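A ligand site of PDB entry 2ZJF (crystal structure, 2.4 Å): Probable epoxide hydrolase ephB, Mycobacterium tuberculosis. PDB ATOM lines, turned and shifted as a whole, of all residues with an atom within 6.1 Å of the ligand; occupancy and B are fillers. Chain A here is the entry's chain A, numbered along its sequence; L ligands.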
ATOM      1  N   PHE A  42      20.584  -2.867 -28.596  1.00  0.00           N
ATOM      2  CA  PHE A  42      19.571  -3.844 -28.183  1.00  0.00           C
ATOM      3  C   PHE A  42      18.620  -4.255 -29.317  1.00  0.00           C
ATOM      4  O   PHE A  42      18.074  -3.402 -30.019  1.00  0.00           O
ATOM      5  CB  PHE A  42      18.731  -3.292 -27.025  1.00  0.00           C
ATOM      6  CG  PHE A  42      17.537  -4.143 -26.666  1.00  0.00           C
ATOM      7  CD1 PHE A  42      16.394  -4.126 -27.458  1.00  0.00           C
ATOM      8  CD2 PHE A  42      17.584  -5.003 -25.571  1.00  0.00           C
ATOM      9  CE1 PHE A  42      15.313  -4.970 -27.176  1.00  0.00           C
ATOM     10  CE2 PHE A  42      16.516  -5.842 -25.284  1.00  0.00           C
ATOM     11  CZ  PHE A  42      15.378  -5.824 -26.093  1.00  0.00           C
ATOM     12  N   PRO A  43      18.428  -5.569 -29.530  1.00  0.00           N
ATOM     13  CA  PRO A  43      19.027  -6.703 -28.829  1.00  0.00           C
ATOM     14  C   PRO A  43      20.028  -7.313 -29.820  1.00  0.00           C
ATOM     15  O   PRO A  43      19.689  -8.211 -30.579  1.00  0.00           O
ATOM     16  CB  PRO A  43      17.822  -7.603 -28.586  1.00  0.00           C
ATOM     17  CG  PRO A  43      17.061  -7.463 -29.883  1.00  0.00           C
ATOM     18  CD  PRO A  43      17.235  -5.995 -30.289  1.00  0.00           C
ATOM     19  N   ASP A 110      22.708   2.367 -31.284  1.00  0.00           N
ATOM     20  CA  ASP A 110      21.586   2.140 -30.376  1.00  0.00           C
ATOM     21  C   ASP A 110      22.049   2.300 -28.928  1.00  0.00           C
ATOM     22  O   ASP A 110      22.622   3.326 -28.576  1.00  0.00           O
ATOM     23  CB  ASP A 110      21.020   0.733 -30.604  1.00  0.00           C
ATOM     24  CG  ASP A 110      19.705   0.532 -29.919  1.00  0.00           C
ATOM     25  OD1 ASP A 110      18.753   1.285 -30.233  1.00  0.00           O
ATOM     26  OD2 ASP A 110      19.619  -0.382 -29.062  1.00  0.00           O
ATOM     27  N   TRP A 111      21.823   1.300 -28.081  1.00  0.00           N
ATOM     28  CA  TRP A 111      22.272   1.404 -26.690  1.00  0.00           C
ATOM     29  C   TRP A 111      23.778   1.601 -26.597  1.00  0.00           C
ATOM     30  O   TRP A 111      24.279   2.186 -25.645  1.00  0.00           O
ATOM     31  CB  TRP A 111      21.851   0.178 -25.881  1.00  0.00           C
ATOM     32  CG  TRP A 111      20.754   0.481 -24.918  1.00  0.00           C
ATOM     33  CD1 TRP A 111      19.441   0.110 -25.006  1.00  0.00           C
ATOM     34  CD2 TRP A 111      20.870   1.253 -23.717  1.00  0.00           C
ATOM     35  NE1 TRP A 111      18.734   0.618 -23.947  1.00  0.00           N
ATOM     36  CE2 TRP A 111      19.585   1.318 -23.132  1.00  0.00           C
ATOM     37  CE3 TRP A 111      21.943   1.898 -23.082  1.00  0.00           C
ATOM     38  CZ2 TRP A 111      19.342   2.007 -21.936  1.00  0.00           C
ATOM     39  CZ3 TRP A 111      21.687   2.582 -21.890  1.00  0.00           C
ATOM     40  CH2 TRP A 111      20.402   2.637 -21.336  1.00  0.00           C
ATOM     41  N   GLY A 112      24.505   1.113 -27.600  1.00  0.00           N
ATOM     42  CA  GLY A 112      25.941   1.302 -27.592  1.00  0.00           C
ATOM     43  C   GLY A 112      26.285   2.788 -27.695  1.00  0.00           C
ATOM     44  O   GLY A 112      27.332   3.224 -27.205  1.00  0.00           O
ATOM     45  N   PRO A 114      24.742   5.772 -26.322  1.00  0.00           N
ATOM     46  CA  PRO A 114      24.892   6.541 -25.079  1.00  0.00           C
ATOM     47  C   PRO A 114      26.171   6.161 -24.362  1.00  0.00           C
ATOM     48  O   PRO A 114      26.814   7.006 -23.724  1.00  0.00           O
ATOM     49  CB  PRO A 114      23.653   6.144 -24.283  1.00  0.00           C
ATOM     50  CG  PRO A 114      22.624   5.903 -25.360  1.00  0.00           C
ATOM     51  CD  PRO A 114      23.415   5.136 -26.395  1.00  0.00           C
ATOM     52  N   VAL A 135      21.077   6.643 -32.259  1.00  0.00           N
ATOM     53  CA  VAL A 135      20.779   7.450 -31.079  1.00  0.00           C
ATOM     54  C   VAL A 135      21.789   8.584 -30.921  1.00  0.00           C
ATOM     55  O   VAL A 135      22.939   8.348 -30.598  1.00  0.00           O
ATOM     56  CB  VAL A 135      20.800   6.586 -29.799  1.00  0.00           C
ATOM     57  CG1 VAL A 135      20.422   7.423 -28.583  1.00  0.00           C
ATOM     58  CG2 VAL A 135      19.842   5.415 -29.948  1.00  0.00           C
ATOM     59  N   VAL A 142      20.300  10.298 -21.873  1.00  0.00           N
ATOM     60  CA  VAL A 142      20.653   8.993 -22.432  1.00  0.00           C
ATOM     61  C   VAL A 142      20.125   8.871 -23.869  1.00  0.00           C
ATOM     62  O   VAL A 142      20.906   8.676 -24.803  1.00  0.00           O
ATOM     63  CB  VAL A 142      20.107   7.846 -21.581  1.00  0.00           C
ATOM     64  CG1 VAL A 142      20.388   6.509 -22.258  1.00  0.00           C
ATOM     65  CG2 VAL A 142      20.745   7.887 -20.204  1.00  0.00           C
ATOM     66  N   ILE A 143      18.819   8.969 -24.034  1.00  0.00           N
ATOM     67  CA  ILE A 143      18.239   8.921 -25.362  1.00  0.00           C
ATOM     68  C   ILE A 143      17.337  10.137 -25.512  1.00  0.00           C
ATOM     69  O   ILE A 143      16.453  10.358 -24.678  1.00  0.00           O
ATOM     70  CB  ILE A 143      17.398   7.664 -25.612  1.00  0.00           C
ATOM     71  CG1 ILE A 143      16.794   7.729 -27.019  1.00  0.00           C
ATOM     72  CG2 ILE A 143      16.299   7.541 -24.567  1.00  0.00           C
ATOM     73  CD1 ILE A 143      16.168   6.433 -27.511  1.00  0.00           C
ATOM     74  N   TYR A 170       6.905   1.417 -24.337  1.00  0.00           N
ATOM     75  CA  TYR A 170       7.643   0.155 -24.391  1.00  0.00           C
ATOM     76  C   TYR A 170       8.852   0.089 -23.439  1.00  0.00           C
ATOM     77  O   TYR A 170       9.117  -0.960 -22.857  1.00  0.00           O
ATOM     78  CB  TYR A 170       8.087  -0.148 -25.824  1.00  0.00           C
ATOM     79  CG  TYR A 170       9.324   0.600 -26.280  1.00  0.00           C
ATOM     80  CD1 TYR A 170       9.284   1.972 -26.527  1.00  0.00           C
ATOM     81  CD2 TYR A 170      10.536  -0.064 -26.447  1.00  0.00           C
ATOM     82  CE1 TYR A 170      10.421   2.661 -26.910  1.00  0.00           C
ATOM     83  CE2 TYR A 170      11.693   0.614 -26.831  1.00  0.00           C
ATOM     84  CZ  TYR A 170      11.625   1.982 -27.062  1.00  0.00           C
ATOM     85  OH  TYR A 170      12.763   2.682 -27.414  1.00  0.00           O
ATOM     86  N   GLN A 171       9.572   1.187 -23.283  1.00  0.00           N
ATOM     87  CA  GLN A 171      10.735   1.200 -22.402  1.00  0.00           C
ATOM     88  C   GLN A 171      10.402   0.901 -20.941  1.00  0.00           C
ATOM     89  O   GLN A 171      11.179   0.245 -20.246  1.00  0.00           O
ATOM     90  CB  GLN A 171      11.461   2.538 -22.515  1.00  0.00           C
ATOM     91  CG  GLN A 171      12.207   2.701 -23.822  1.00  0.00           C
ATOM     92  CD  GLN A 171      12.799   4.081 -24.008  1.00  0.00           C
ATOM     93  OE1 GLN A 171      13.127   4.769 -23.041  1.00  0.00           O
ATOM     94  NE2 GLN A 171      12.955   4.484 -25.266  1.00  0.00           N
ATOM     95  N   PHE A 174       9.746  -2.746 -20.859  1.00  0.00           N
ATOM     96  CA  PHE A 174      11.028  -3.420 -20.899  1.00  0.00           C
ATOM     97  C   PHE A 174      11.634  -3.442 -19.500  1.00  0.00           C
ATOM     98  O   PHE A 174      12.144  -4.454 -19.059  1.00  0.00           O
ATOM     99  CB  PHE A 174      12.003  -2.692 -21.847  1.00  0.00           C
ATOM    100  CG  PHE A 174      11.872  -3.088 -23.297  1.00  0.00           C
ATOM    101  CD1 PHE A 174      10.713  -3.695 -23.782  1.00  0.00           C
ATOM    102  CD2 PHE A 174      12.908  -2.822 -24.188  1.00  0.00           C
ATOM    103  CE1 PHE A 174      10.598  -4.032 -25.137  1.00  0.00           C
ATOM    104  CE2 PHE A 174      12.804  -3.146 -25.544  1.00  0.00           C
ATOM    105  CZ  PHE A 174      11.646  -3.761 -26.023  1.00  0.00           C
ATOM    106  N   LEU A 195      10.503  -7.939 -34.148  1.00  0.00           N
ATOM    107  CA  LEU A 195      11.109  -6.661 -33.781  1.00  0.00           C
ATOM    108  C   LEU A 195      12.027  -6.123 -34.877  1.00  0.00           C
ATOM    109  O   LEU A 195      11.918  -4.954 -35.270  1.00  0.00           O
ATOM    110  CB  LEU A 195      11.928  -6.824 -32.490  1.00  0.00           C
ATOM    111  CG  LEU A 195      12.516  -5.516 -31.926  1.00  0.00           C
ATOM    112  CD1 LEU A 195      11.387  -4.700 -31.312  1.00  0.00           C
ATOM    113  CD2 LEU A 195      13.579  -5.809 -30.885  1.00  0.00           C
ATOM    114  N   VAL A 199      10.804  -2.351 -37.061  1.00  0.00           N
ATOM    115  CA  VAL A 199      11.520  -1.081 -37.077  1.00  0.00           C
ATOM    116  C   VAL A 199      12.523  -0.927 -38.201  1.00  0.00           C
ATOM    117  O   VAL A 199      13.197   0.092 -38.297  1.00  0.00           O
ATOM    118  CB  VAL A 199      12.250  -0.799 -35.727  1.00  0.00           C
ATOM    119  CG1 VAL A 199      11.238  -0.656 -34.606  1.00  0.00           C
ATOM    120  CG2 VAL A 199      13.252  -1.917 -35.426  1.00  0.00           C
ATOM    121  N   LEU A 232       5.615   0.984 -30.940  1.00  0.00           N
ATOM    122  CA  LEU A 232       6.194   0.909 -29.608  1.00  0.00           C
ATOM    123  C   LEU A 232       5.317   1.556 -28.537  1.00  0.00           C
ATOM    124  O   LEU A 232       5.726   1.663 -27.372  1.00  0.00           O
ATOM    125  CB  LEU A 232       7.587   1.547 -29.628  1.00  0.00           C
ATOM    126  CG  LEU A 232       8.502   0.915 -30.687  1.00  0.00           C
ATOM    127  CD1 LEU A 232       9.864   1.571 -30.642  1.00  0.00           C
ATOM    128  CD2 LEU A 232       8.631  -0.578 -30.448  1.00  0.00           C
ATOM    129  N   TYR A 278      17.657  -0.764 -19.768  1.00  0.00           N
ATOM    130  CA  TYR A 278      16.457   0.071 -19.726  1.00  0.00           C
ATOM    131  C   TYR A 278      16.044   0.385 -18.301  1.00  0.00           C
ATOM    132  O   TYR A 278      15.746   1.532 -17.947  1.00  0.00           O
ATOM    133  CB  TYR A 278      15.295  -0.629 -20.456  1.00  0.00           C
ATOM    134  CG  TYR A 278      15.496  -0.729 -21.964  1.00  0.00           C
ATOM    135  CD1 TYR A 278      14.919   0.204 -22.823  1.00  0.00           C
ATOM    136  CD2 TYR A 278      16.276  -1.746 -22.507  1.00  0.00           C
ATOM    137  CE1 TYR A 278      15.129   0.132 -24.210  1.00  0.00           C
ATOM    138  CE2 TYR A 278      16.500  -1.829 -23.878  1.00  0.00           C
ATOM    139  CZ  TYR A 278      15.927  -0.890 -24.729  1.00  0.00           C
ATOM    140  OH  TYR A 278      16.179  -0.958 -26.083  1.00  0.00           O
ATOM    141  N   ILE A 281      17.543   3.518 -16.894  1.00  0.00           N
ATOM    142  CA  ILE A 281      17.478   4.814 -17.563  1.00  0.00           C
ATOM    143  C   ILE A 281      17.364   5.974 -16.560  1.00  0.00           C
ATOM    144  O   ILE A 281      18.193   6.864 -16.552  1.00  0.00           O
ATOM    145  CB  ILE A 281      16.313   4.858 -18.569  1.00  0.00           C
ATOM    146  CG1 ILE A 281      16.638   3.948 -19.758  1.00  0.00           C
ATOM    147  CG2 ILE A 281      16.080   6.286 -19.047  1.00  0.00           C
ATOM    148  CD1 ILE A 281      15.544   3.825 -20.781  1.00  0.00           C
ATOM    149  N   VAL A 309      13.664   5.036 -35.788  1.00  0.00           N
ATOM    150  CA  VAL A 309      12.969   5.694 -34.679  1.00  0.00           C
ATOM    151  C   VAL A 309      13.958   6.469 -33.819  1.00  0.00           C
ATOM    152  O   VAL A 309      13.639   7.544 -33.306  1.00  0.00           O
ATOM    153  CB  VAL A 309      12.204   4.669 -33.795  1.00  0.00           C
ATOM    154  CG1 VAL A 309      11.082   4.028 -34.587  1.00  0.00           C
ATOM    155  CG2 VAL A 309      13.168   3.601 -33.266  1.00  0.00           C
ATOM    156  N   TRP A 313      13.160  10.289 -33.159  1.00  0.00           N
ATOM    157  CA  TRP A 313      12.912  10.780 -31.806  1.00  0.00           C
ATOM    158  C   TRP A 313      13.967  11.765 -31.349  1.00  0.00           C
ATOM    159  O   TRP A 313      13.679  12.683 -30.580  1.00  0.00           O
ATOM    160  CB  TRP A 313      12.834   9.625 -30.803  1.00  0.00           C
ATOM    161  CG  TRP A 313      11.748   8.617 -31.082  1.00  0.00           C
ATOM    162  CD1 TRP A 313      10.569   8.838 -31.727  1.00  0.00           C
ATOM    163  CD2 TRP A 313      11.732   7.242 -30.678  1.00  0.00           C
ATOM    164  NE1 TRP A 313       9.817   7.687 -31.763  1.00  0.00           N
ATOM    165  CE2 TRP A 313      10.516   6.690 -31.130  1.00  0.00           C
ATOM    166  CE3 TRP A 313      12.634   6.417 -29.995  1.00  0.00           C
ATOM    167  CZ2 TRP A 313      10.174   5.355 -30.906  1.00  0.00           C
ATOM    168  CZ3 TRP A 313      12.294   5.096 -29.770  1.00  0.00           C
ATOM    169  CH2 TRP A 313      11.073   4.573 -30.215  1.00  0.00           C
ATOM    170  N   HIS A 339      16.079   1.327 -38.424  1.00  0.00           N
ATOM    171  CA  HIS A 339      16.876   1.270 -37.207  1.00  0.00           C
ATOM    172  C   HIS A 339      18.223   0.544 -37.259  1.00  0.00           C
ATOM    173  O   HIS A 339      19.207   1.014 -36.677  1.00  0.00           O
ATOM    174  CB  HIS A 339      16.045   0.665 -36.080  1.00  0.00           C
ATOM    175  CG  HIS A 339      16.769   0.581 -34.786  1.00  0.00           C
ATOM    176  ND1 HIS A 339      17.151   1.701 -34.071  1.00  0.00           N
ATOM    177  CD2 HIS A 339      17.226  -0.488 -34.092  1.00  0.00           C
ATOM    178  CE1 HIS A 339      17.808   1.319 -32.984  1.00  0.00           C
ATOM    179  NE2 HIS A 339      17.864   0.000 -32.972  1.00  0.00           N
ATOM    180  N   TRP A 340      18.252  -0.598 -37.935  1.00  0.00           N
ATOM    181  CA  TRP A 340      19.467  -1.404 -38.006  1.00  0.00           C
ATOM    182  C   TRP A 340      20.426  -0.883 -39.065  1.00  0.00           C
ATOM    183  O   TRP A 340      20.834  -1.584 -39.999  1.00  0.00           O
ATOM    184  CB  TRP A 340      19.056  -2.860 -38.259  1.00  0.00           C
ATOM    185  CG  TRP A 340      17.826  -3.202 -37.456  1.00  0.00           C
ATOM    186  CD1 TRP A 340      16.527  -3.218 -37.895  1.00  0.00           C
ATOM    187  CD2 TRP A 340      17.769  -3.451 -36.039  1.00  0.00           C
ATOM    188  NE1 TRP A 340      15.671  -3.457 -36.844  1.00  0.00           N
ATOM    189  CE2 TRP A 340      16.403  -3.612 -35.698  1.00  0.00           C
ATOM    190  CE3 TRP A 340      18.727  -3.567 -35.029  1.00  0.00           C
ATOM    191  CZ2 TRP A 340      15.976  -3.859 -34.387  1.00  0.00           C
ATOM    192  CZ3 TRP A 340      18.318  -3.815 -33.724  1.00  0.00           C
ATOM    193  CH2 TRP A 340      16.944  -3.964 -33.415  1.00  0.00           C
HETATM  194  N1  LIG L   1      16.088   0.579 -29.235  1.00  0.00           N
HETATM  195  C1  LIG L   1      15.994   1.373 -28.140  1.00  0.00           C
HETATM  196  N2  LIG L   1      17.184   1.885 -27.755  1.00  0.00           N
HETATM  197  O1  LIG L   1      14.935   1.585 -27.561  1.00  0.00           O
HETATM  198  C2  LIG L   1      15.123  -0.091 -29.922  1.00  0.00           C
HETATM  199  C3  LIG L   1      15.618  -0.856 -31.026  1.00  0.00           C
HETATM  200  C4  LIG L   1      14.719  -1.622 -31.837  1.00  0.00           C
HETATM  201  C5  LIG L   1      13.318  -1.615 -31.533  1.00  0.00           C
HETATM  202  C6  LIG L   1      12.808  -0.860 -30.440  1.00  0.00           C
HETATM  203  C7  LIG L   1      13.708  -0.102 -29.624  1.00  0.00           C
HETATM  204  C8  LIG L   1      17.470   2.707 -26.701  1.00  0.00           C
HETATM  205  C9  LIG L   1      16.542   3.234 -25.715  1.00  0.00           C
HETATM  206  C10 LIG L   1      16.979   4.076 -24.658  1.00  0.00           C
HETATM  207  C11 LIG L   1      18.375   4.412 -24.563  1.00  0.00           C
HETATM  208  C12 LIG L   1      19.322   3.893 -25.523  1.00  0.00           C
HETATM  209  C13 LIG L   1      18.864   3.048 -26.582  1.00  0.00           C
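The side-chain hydroxyl (OH) of Tyr 170 sits at hydrogen-bond distance from an oxygen (O1) of the ligand (2.4 Å).
The side-chain carboxylate of Asp 110 sits at hydrogen-bond distance from a nitrogen (N1) of the ligand.
O1 of the ligand sits close to OH of Tyr 278, at 3.2 Å.
The side-chain carboxylate (OD2) of Asp 110 is in hydrogen-bond range of the backbone NH (N) of Phe 42, at 2.7 Å.
The backbone carbonyl oxygen (O) of Leu 232 is in hydrogen-bond range of the backbone NH (N) of Tyr 170, 3.3 Å away.
OH of Tyr 170 lies within hydrogen-bond range of NE2 of Gln 171, 2.8 Å away.
N of His 339 sits at hydrogen-bond distance from O of Val 199, 3.1 Å away.
The side-chain carboxylate (OD1) of Asp 110 sits close to a ring nitrogen (NE2) of His 339, 3.2 Å away.
Phe 42 touches the ligand (O to C3, 3.7 Å).
CD1 of Trp 111 touches C13 of the ligand, at 3.4 Å.
Pro 114 touches the ligand (CG to C12, 3.9 Å).
CG1 of Val 142 touches C11 of the ligand, 3.7 Å away.
CG2 of Ile 143 touches C10 of the ligand, 3.5 Å away.
Gln 171 touches the ligand.
CD1 of Leu 195 touches C5 of the ligand, 3.6 Å away.
Val 199 touches the ligand (CG1 to C5, 3.8 Å).
CD1 of Leu 232 touches C6 of the ligand (3.8 Å).
NE2 of His 339 touches C3 of the ligand, 3.1 Å away.
Trp 340 touches the ligand.
Along chain A the residues within 4 Å of the ligand span positions 42 to 340.
The nearest printed residue that does not touch the ligand is Ile 281 (4.1 Å).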
